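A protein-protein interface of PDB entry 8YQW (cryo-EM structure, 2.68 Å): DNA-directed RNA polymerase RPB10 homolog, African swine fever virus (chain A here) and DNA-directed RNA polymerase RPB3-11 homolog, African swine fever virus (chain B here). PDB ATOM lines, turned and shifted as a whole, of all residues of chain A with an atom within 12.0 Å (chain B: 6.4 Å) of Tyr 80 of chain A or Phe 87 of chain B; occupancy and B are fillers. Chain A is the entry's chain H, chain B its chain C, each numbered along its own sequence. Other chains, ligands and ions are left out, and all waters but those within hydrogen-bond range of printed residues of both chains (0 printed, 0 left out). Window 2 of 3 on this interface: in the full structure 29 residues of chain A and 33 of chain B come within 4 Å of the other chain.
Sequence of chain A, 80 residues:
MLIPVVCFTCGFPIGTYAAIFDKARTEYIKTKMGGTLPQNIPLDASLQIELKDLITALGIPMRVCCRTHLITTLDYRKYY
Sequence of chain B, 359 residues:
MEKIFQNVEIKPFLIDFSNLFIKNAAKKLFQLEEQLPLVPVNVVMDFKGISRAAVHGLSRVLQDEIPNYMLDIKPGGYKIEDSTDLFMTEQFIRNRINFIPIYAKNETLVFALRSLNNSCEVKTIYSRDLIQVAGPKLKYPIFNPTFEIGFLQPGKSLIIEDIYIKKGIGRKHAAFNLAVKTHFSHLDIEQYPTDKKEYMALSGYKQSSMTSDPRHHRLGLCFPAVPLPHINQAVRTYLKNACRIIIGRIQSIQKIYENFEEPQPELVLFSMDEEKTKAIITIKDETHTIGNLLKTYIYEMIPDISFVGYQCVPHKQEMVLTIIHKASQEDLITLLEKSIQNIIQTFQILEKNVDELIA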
ATOM      1  N   MET A   1     -22.784  -2.900  24.317  1.00  0.00           N
ATOM      2  CA  MET A   1     -22.007  -4.017  24.832  1.00  0.00           C
ATOM      3  C   MET A   1     -20.820  -4.318  23.925  1.00  0.00           C
ATOM      4  O   MET A   1     -19.957  -5.122  24.265  1.00  0.00           O
ATOM      5  CB  MET A   1     -22.891  -5.254  24.984  1.00  0.00           C
ATOM      6  CG  MET A   1     -23.903  -5.156  26.111  1.00  0.00           C
ATOM      7  SD  MET A   1     -24.598  -6.754  26.566  1.00  0.00           S
ATOM      8  CE  MET A   1     -25.967  -6.862  25.423  1.00  0.00           C
ATOM      9  N   LEU A   2     -20.784  -3.665  22.766  1.00  0.00           N
ATOM     10  CA  LEU A   2     -19.688  -3.796  21.819  1.00  0.00           C
ATOM     11  C   LEU A   2     -19.423  -2.442  21.184  1.00  0.00           C
ATOM     12  O   LEU A   2     -20.175  -1.484  21.378  1.00  0.00           O
ATOM     13  CB  LEU A   2     -19.993  -4.828  20.727  1.00  0.00           C
ATOM     14  CG  LEU A   2     -20.313  -6.266  21.117  1.00  0.00           C
ATOM     15  CD1 LEU A   2     -21.048  -6.962  19.991  1.00  0.00           C
ATOM     16  CD2 LEU A   2     -19.039  -7.005  21.460  1.00  0.00           C
ATOM     17  N   LEU A  74     -16.878   0.606  25.698  1.00  0.00           N
ATOM     18  CA  LEU A  74     -16.606  -0.546  26.543  1.00  0.00           C
ATOM     19  C   LEU A  74     -17.088  -1.828  25.879  1.00  0.00           C
ATOM     20  O   LEU A  74     -18.052  -1.832  25.110  1.00  0.00           O
ATOM     21  CB  LEU A  74     -17.282  -0.394  27.904  1.00  0.00           C
ATOM     22  CG  LEU A  74     -17.007   0.864  28.724  1.00  0.00           C
ATOM     23  CD1 LEU A  74     -17.803   0.824  30.012  1.00  0.00           C
ATOM     24  CD2 LEU A  74     -15.528   1.010  29.013  1.00  0.00           C
ATOM     25  N   ASP A  75     -16.409  -2.926  26.190  1.00  0.00           N
ATOM     26  CA  ASP A  75     -16.731  -4.239  25.650  1.00  0.00           C
ATOM     27  C   ASP A  75     -17.243  -5.120  26.781  1.00  0.00           C
ATOM     28  O   ASP A  75     -16.551  -5.310  27.784  1.00  0.00           O
ATOM     29  CB  ASP A  75     -15.507  -4.864  24.984  1.00  0.00           C
ATOM     30  CG  ASP A  75     -15.866  -5.999  24.056  1.00  0.00           C
ATOM     31  OD1 ASP A  75     -17.050  -6.378  24.010  1.00  0.00           O
ATOM     32  OD2 ASP A  75     -14.964  -6.510  23.365  1.00  0.00           O
ATOM     33  N   TYR A  76     -18.452  -5.656  26.615  1.00  0.00           N
ATOM     34  CA  TYR A  76     -19.052  -6.473  27.663  1.00  0.00           C
ATOM     35  C   TYR A  76     -18.329  -7.802  27.832  1.00  0.00           C
ATOM     36  O   TYR A  76     -18.321  -8.363  28.933  1.00  0.00           O
ATOM     37  CB  TYR A  76     -20.527  -6.710  27.358  1.00  0.00           C
ATOM     38  CG  TYR A  76     -21.370  -7.078  28.555  1.00  0.00           C
ATOM     39  CD1 TYR A  76     -21.959  -6.101  29.338  1.00  0.00           C
ATOM     40  CD2 TYR A  76     -21.598  -8.404  28.887  1.00  0.00           C
ATOM     41  CE1 TYR A  76     -22.736  -6.429  30.422  1.00  0.00           C
ATOM     42  CE2 TYR A  76     -22.376  -8.741  29.973  1.00  0.00           C
ATOM     43  CZ  TYR A  76     -22.942  -7.749  30.734  1.00  0.00           C
ATOM     44  OH  TYR A  76     -23.717  -8.079  31.815  1.00  0.00           O
ATOM     45  N   ARG A  77     -17.729  -8.326  26.761  1.00  0.00           N
ATOM     46  CA  ARG A  77     -17.001  -9.585  26.867  1.00  0.00           C
ATOM     47  C   ARG A  77     -15.807  -9.463  27.800  1.00  0.00           C
ATOM     48  O   ARG A  77     -15.394 -10.454  28.413  1.00  0.00           O
ATOM     49  CB  ARG A  77     -16.531 -10.045  25.489  1.00  0.00           C
ATOM     50  CG  ARG A  77     -17.638 -10.313  24.501  1.00  0.00           C
ATOM     51  CD  ARG A  77     -17.078 -10.513  23.108  1.00  0.00           C
ATOM     52  NE  ARG A  77     -16.632  -9.258  22.515  1.00  0.00           N
ATOM     53  CZ  ARG A  77     -16.173  -9.135  21.278  1.00  0.00           C
ATOM     54  NH1 ARG A  77     -16.091 -10.175  20.466  1.00  0.00           N
ATOM     55  NH2 ARG A  77     -15.783  -7.940  20.848  1.00  0.00           N
ATOM     56  N   LYS A  78     -15.242  -8.266  27.922  1.00  0.00           N
ATOM     57  CA  LYS A  78     -14.034  -8.050  28.701  1.00  0.00           C
ATOM     58  C   LYS A  78     -14.307  -7.738  30.165  1.00  0.00           C
ATOM     59  O   LYS A  78     -13.356  -7.630  30.945  1.00  0.00           O
ATOM     60  CB  LYS A  78     -13.216  -6.920  28.075  1.00  0.00           C
ATOM     61  CG  LYS A  78     -12.683  -7.262  26.698  1.00  0.00           C
ATOM     62  CD  LYS A  78     -12.089  -6.055  26.010  1.00  0.00           C
ATOM     63  CE  LYS A  78     -11.476  -6.438  24.680  1.00  0.00           C
ATOM     64  NZ  LYS A  78     -10.892  -5.262  23.986  1.00  0.00           N
ATOM     65  N   TYR A  79     -15.571  -7.589  30.559  1.00  0.00           N
ATOM     66  CA  TYR A  79     -15.931  -7.352  31.947  1.00  0.00           C
ATOM     67  C   TYR A  79     -16.778  -8.466  32.536  1.00  0.00           C
ATOM     68  O   TYR A  79     -17.140  -8.388  33.714  1.00  0.00           O
ATOM     69  CB  TYR A  79     -16.685  -6.024  32.091  1.00  0.00           C
ATOM     70  CG  TYR A  79     -15.851  -4.805  31.804  1.00  0.00           C
ATOM     71  CD1 TYR A  79     -15.016  -4.272  32.770  1.00  0.00           C
ATOM     72  CD2 TYR A  79     -15.905  -4.182  30.570  1.00  0.00           C
ATOM     73  CE1 TYR A  79     -14.255  -3.154  32.513  1.00  0.00           C
ATOM     74  CE2 TYR A  79     -15.148  -3.066  30.303  1.00  0.00           C
ATOM     75  CZ  TYR A  79     -14.325  -2.554  31.279  1.00  0.00           C
ATOM     76  OH  TYR A  79     -13.566  -1.438  31.018  1.00  0.00           O
ATOM     77  N   TYR A  80     -17.109  -9.488  31.758  1.00  0.00           N
ATOM     78  CA  TYR A  80     -17.998 -10.544  32.215  1.00  0.00           C
ATOM     79  C   TYR A  80     -17.441 -11.921  31.876  1.00  0.00           C
ATOM     80  O   TYR A  80     -17.432 -12.331  30.716  1.00  0.00           O
ATOM     81  CB  TYR A  80     -19.384 -10.368  31.598  1.00  0.00           C
ATOM     82  CG  TYR A  80     -20.430 -11.292  32.167  1.00  0.00           C
ATOM     83  CD1 TYR A  80     -20.941 -11.095  33.437  1.00  0.00           C
ATOM     84  CD2 TYR A  80     -20.909 -12.362  31.431  1.00  0.00           C
ATOM     85  CE1 TYR A  80     -21.895 -11.938  33.958  1.00  0.00           C
ATOM     86  CE2 TYR A  80     -21.862 -13.208  31.946  1.00  0.00           C
ATOM     87  CZ  TYR A  80     -22.353 -12.990  33.209  1.00  0.00           C
ATOM     88  OH  TYR A  80     -23.306 -13.830  33.731  1.00  0.00           O
ATOM     89  N   THR B  84     -31.102 -19.457  23.014  1.00  0.00           N
ATOM     90  CA  THR B  84     -30.971 -19.629  24.452  1.00  0.00           C
ATOM     91  C   THR B  84     -30.106 -18.565  25.113  1.00  0.00           C
ATOM     92  O   THR B  84     -30.073 -18.499  26.346  1.00  0.00           O
ATOM     93  CB  THR B  84     -30.388 -21.008  24.776  1.00  0.00           C
ATOM     94  OG1 THR B  84     -29.148 -21.176  24.085  1.00  0.00           O
ATOM     95  CG2 THR B  84     -31.348 -22.102  24.356  1.00  0.00           C
ATOM     96  N   ASP B  85     -29.412 -17.736  24.338  1.00  0.00           N
ATOM     97  CA  ASP B  85     -28.501 -16.767  24.930  1.00  0.00           C
ATOM     98  C   ASP B  85     -29.280 -15.694  25.674  1.00  0.00           C
ATOM     99  O   ASP B  85     -30.237 -15.121  25.145  1.00  0.00           O
ATOM    100  CB  ASP B  85     -27.616 -16.129  23.866  1.00  0.00           C
ATOM    101  CG  ASP B  85     -26.474 -15.336  24.469  1.00  0.00           C
ATOM    102  OD1 ASP B  85     -25.494 -15.958  24.926  1.00  0.00           O
ATOM    103  OD2 ASP B  85     -26.558 -14.093  24.498  1.00  0.00           O
ATOM    104  N   LEU B  86     -28.855 -15.419  26.903  1.00  0.00           N
ATOM    105  CA  LEU B  86     -29.562 -14.504  27.783  1.00  0.00           C
ATOM    106  C   LEU B  86     -29.177 -13.048  27.572  1.00  0.00           C
ATOM    107  O   LEU B  86     -29.959 -12.160  27.927  1.00  0.00           O
ATOM    108  CB  LEU B  86     -29.303 -14.890  29.240  1.00  0.00           C
ATOM    109  CG  LEU B  86     -29.742 -16.286  29.677  1.00  0.00           C
ATOM    110  CD1 LEU B  86     -29.476 -16.478  31.158  1.00  0.00           C
ATOM    111  CD2 LEU B  86     -31.206 -16.513  29.358  1.00  0.00           C
ATOM    112  N   PHE B  87     -28.002 -12.780  27.011  1.00  0.00           N
ATOM    113  CA  PHE B  87     -27.523 -11.415  26.849  1.00  0.00           C
ATOM    114  C   PHE B  87     -27.778 -10.849  25.462  1.00  0.00           C
ATOM    115  O   PHE B  87     -27.892  -9.627  25.318  1.00  0.00           O
ATOM    116  CB  PHE B  87     -26.025 -11.344  27.163  1.00  0.00           C
ATOM    117  CG  PHE B  87     -25.689 -11.726  28.573  1.00  0.00           C
ATOM    118  CD1 PHE B  87     -25.675 -10.775  29.576  1.00  0.00           C
ATOM    119  CD2 PHE B  87     -25.402 -13.039  28.902  1.00  0.00           C
ATOM    120  CE1 PHE B  87     -25.375 -11.125  30.874  1.00  0.00           C
ATOM    121  CE2 PHE B  87     -25.103 -13.392  30.197  1.00  0.00           C
ATOM    122  CZ  PHE B  87     -25.091 -12.432  31.184  1.00  0.00           C
ATOM    123  N   MET B  88     -27.878 -11.696  24.438  1.00  0.00           N
ATOM    124  CA  MET B  88     -28.153 -11.233  23.080  1.00  0.00           C
ATOM    125  C   MET B  88     -29.664 -11.156  22.893  1.00  0.00           C
ATOM    126  O   MET B  88     -30.315 -12.073  22.391  1.00  0.00           O
ATOM    127  CB  MET B  88     -27.499 -12.148  22.053  1.00  0.00           C
ATOM    128  CG  MET B  88     -25.989 -12.031  22.007  1.00  0.00           C
ATOM    129  SD  MET B  88     -25.409 -10.350  21.734  1.00  0.00           S
ATOM    130  CE  MET B  88     -24.711  -9.963  23.332  1.00  0.00           C
ATOM    131  N   THR B  89     -30.225 -10.027  23.313  1.00  0.00           N
ATOM    132  CA  THR B  89     -31.656  -9.805  23.200  1.00  0.00           C
ATOM    133  C   THR B  89     -32.021  -9.420  21.768  1.00  0.00           C
ATOM    134  O   THR B  89     -31.162  -9.134  20.934  1.00  0.00           O
ATOM    135  CB  THR B  89     -32.109  -8.726  24.179  1.00  0.00           C
ATOM    136  OG1 THR B  89     -31.484  -7.483  23.846  1.00  0.00           O
ATOM    137  CG2 THR B  89     -31.726  -9.107  25.595  1.00  0.00           C
ATOM    138  N   PHE B  92     -31.141  -5.619  20.967  1.00  0.00           N
ATOM    139  CA  PHE B  92     -29.720  -5.383  20.731  1.00  0.00           C
ATOM    140  C   PHE B  92     -29.293  -5.890  19.359  1.00  0.00           C
ATOM    141  O   PHE B  92     -28.683  -5.155  18.572  1.00  0.00           O
ATOM    142  CB  PHE B  92     -28.903  -6.053  21.838  1.00  0.00           C
ATOM    143  CG  PHE B  92     -27.430  -5.771  21.766  1.00  0.00           C
ATOM    144  CD1 PHE B  92     -26.926  -4.549  22.168  1.00  0.00           C
ATOM    145  CD2 PHE B  92     -26.552  -6.733  21.304  1.00  0.00           C
ATOM    146  CE1 PHE B  92     -25.577  -4.292  22.105  1.00  0.00           C
ATOM    147  CE2 PHE B  92     -25.202  -6.478  21.240  1.00  0.00           C
ATOM    148  CZ  PHE B  92     -24.714  -5.257  21.640  1.00  0.00           C
ATOM    149  N   VAL B 122     -16.475 -17.903  25.151  1.00  0.00           N
ATOM    150  CA  VAL B 122     -17.451 -17.049  24.487  1.00  0.00           C
ATOM    151  C   VAL B 122     -17.121 -16.962  23.006  1.00  0.00           C
ATOM    152  O   VAL B 122     -15.961 -16.769  22.622  1.00  0.00           O
ATOM    153  CB  VAL B 122     -17.470 -15.662  25.146  1.00  0.00           C
ATOM    154  CG1 VAL B 122     -18.370 -14.712  24.382  1.00  0.00           C
ATOM    155  CG2 VAL B 122     -17.912 -15.776  26.592  1.00  0.00           C
ATOM    156  N   PHE B 151     -22.217 -11.889  20.557  1.00  0.00           N
ATOM    157  CA  PHE B 151     -21.385 -12.908  21.179  1.00  0.00           C
ATOM    158  C   PHE B 151     -22.258 -13.809  22.038  1.00  0.00           C
ATOM    159  O   PHE B 151     -23.219 -13.348  22.658  1.00  0.00           O
ATOM    160  CB  PHE B 151     -20.253 -12.299  22.019  1.00  0.00           C
ATOM    161  CG  PHE B 151     -20.711 -11.288  23.028  1.00  0.00           C
ATOM    162  CD1 PHE B 151     -20.836  -9.956  22.683  1.00  0.00           C
ATOM    163  CD2 PHE B 151     -20.996 -11.667  24.327  1.00  0.00           C
ATOM    164  CE1 PHE B 151     -21.250  -9.024  23.612  1.00  0.00           C
ATOM    165  CE2 PHE B 151     -21.410 -10.739  25.257  1.00  0.00           C
ATOM    166  CZ  PHE B 151     -21.537  -9.416  24.899  1.00  0.00           C
ATOM    167  N   GLN B 153     -22.417 -16.737  25.121  1.00  0.00           N
ATOM    168  CA  GLN B 153     -21.804 -17.399  26.253  1.00  0.00           C
ATOM    169  C   GLN B 153     -21.677 -18.890  25.957  1.00  0.00           C
ATOM    170  O   GLN B 153     -22.349 -19.410  25.064  1.00  0.00           O
ATOM    171  CB  GLN B 153     -22.640 -17.170  27.508  1.00  0.00           C
ATOM    172  CG  GLN B 153     -22.876 -15.709  27.838  1.00  0.00           C
ATOM    173  CD  GLN B 153     -21.606 -14.987  28.221  1.00  0.00           C
ATOM    174  OE1 GLN B 153     -20.846 -15.452  29.066  1.00  0.00           O
ATOM    175  NE2 GLN B 153     -21.365 -13.844  27.593  1.00  0.00           N
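Of the printed residues of chain B, Leu 2 of chain A touches Phe 151. Printed residues of chain B within 4 Å of Tyr 76 of chain A: Phe 87 (3.6 Å) and Phe 151 (3.8 Å). Tyr 80 of chain A touches two residues of chain B. Thr 84 of chain B touches none of the printed residues of chain A. No residue of chain A comes within 4 Å of Asp 85 of chain B. No residue of chain A comes within 4 Å of Leu 86 of chain B. Phe 87 of chain B touches just these residues of chain A: Met 1 (3.4 Å), Tyr 76 (3.6 Å) and Tyr 80 (3.4 Å). Of the printed residues of chain A, Phe 92 of chain B touches Met 1. Printed residues of chain A within 4 Å of Phe 151 of chain B: Leu 2, Tyr 76 and Arg 77. Printed residues of chain A within 4 Å of Gln 153 of chain B: Tyr 80. The nearest residue of chain B that does not touch Tyr 80 of chain A is Val 122 of chain B (5.4 Å).
The side-chain carboxylate (OD2) of Asp 85 of chain B lies within hydrogen-bond range of the backbone NH (N) of Met 88 of chain B (2.7 Å). The side-chain carboxylate of Asp 75 of chain A lies within salt-bridge range of the guanidinium group of Arg 77 of chain A, 3.0 Å away. The side-chain sulfur (SD) of Met 88 of chain B is in hydrogen-bond range of the backbone NH (N) of Phe 151 of chain B (3.7 Å). The backbone NH (N) of Gln 153 of chain B sits at hydrogen-bond distance from the side-chain carboxylate (OD1) of Asp 85 of chain B. The side-chain carboxylate (OD2) of Asp 85 of chain B lies within hydrogen-bond range of the backbone NH (N) of Phe 87 of chain B (3.2 Å). OG1 of Thr 89 of chain B is in hydrogen-bond range of N of Phe 92 of chain B (3.4 Å).
CE of Met 1 of chain A touches O of Phe 87 of chain B (3.4 Å). CE of Met 1 of chain A touches CE of Met 88 of chain B, at 3.9 Å. Met 1 of chain A touches Phe 92 of chain B (CB to CZ, 3.8 Å). CD1 of Phe 151 of chain B touches CD2 of Leu 2 of chain A, at 3.7 Å. CE1 of Phe 87 of chain B touches OH of Tyr 76 of chain A, at 3.6 Å. CB of Tyr 76 of chain A touches CZ of Phe 151 of chain B, 3.8 Å away. Arg 77 of chain A touches Phe 151 of chain B (CG to CG, 3.5 Å). CZ of Phe 87 of chain B touches CE2 of Tyr 80 of chain A (3.4 Å). Gln 153 of chain B touches Tyr 80 of chain A (OE1 to CE2, 3.8 Å).
Hydrophobic or aromatic side chains of chain B that line the printed part of chain A: Phe 87, Met 88, Phe 92 and Phe 151. Along chain B the printed residues that touch a printed residue of chain A span positions 87 to 153. Of the 9 printed residues of chain A, 5 touch a printed residue of chain B. Hydrophobic or aromatic side chains of chain A that line the printed part of chain B: Met 1, Leu 2, Tyr 76 and Tyr 80. Among the printed residues, 9 pairs touch across the chains.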
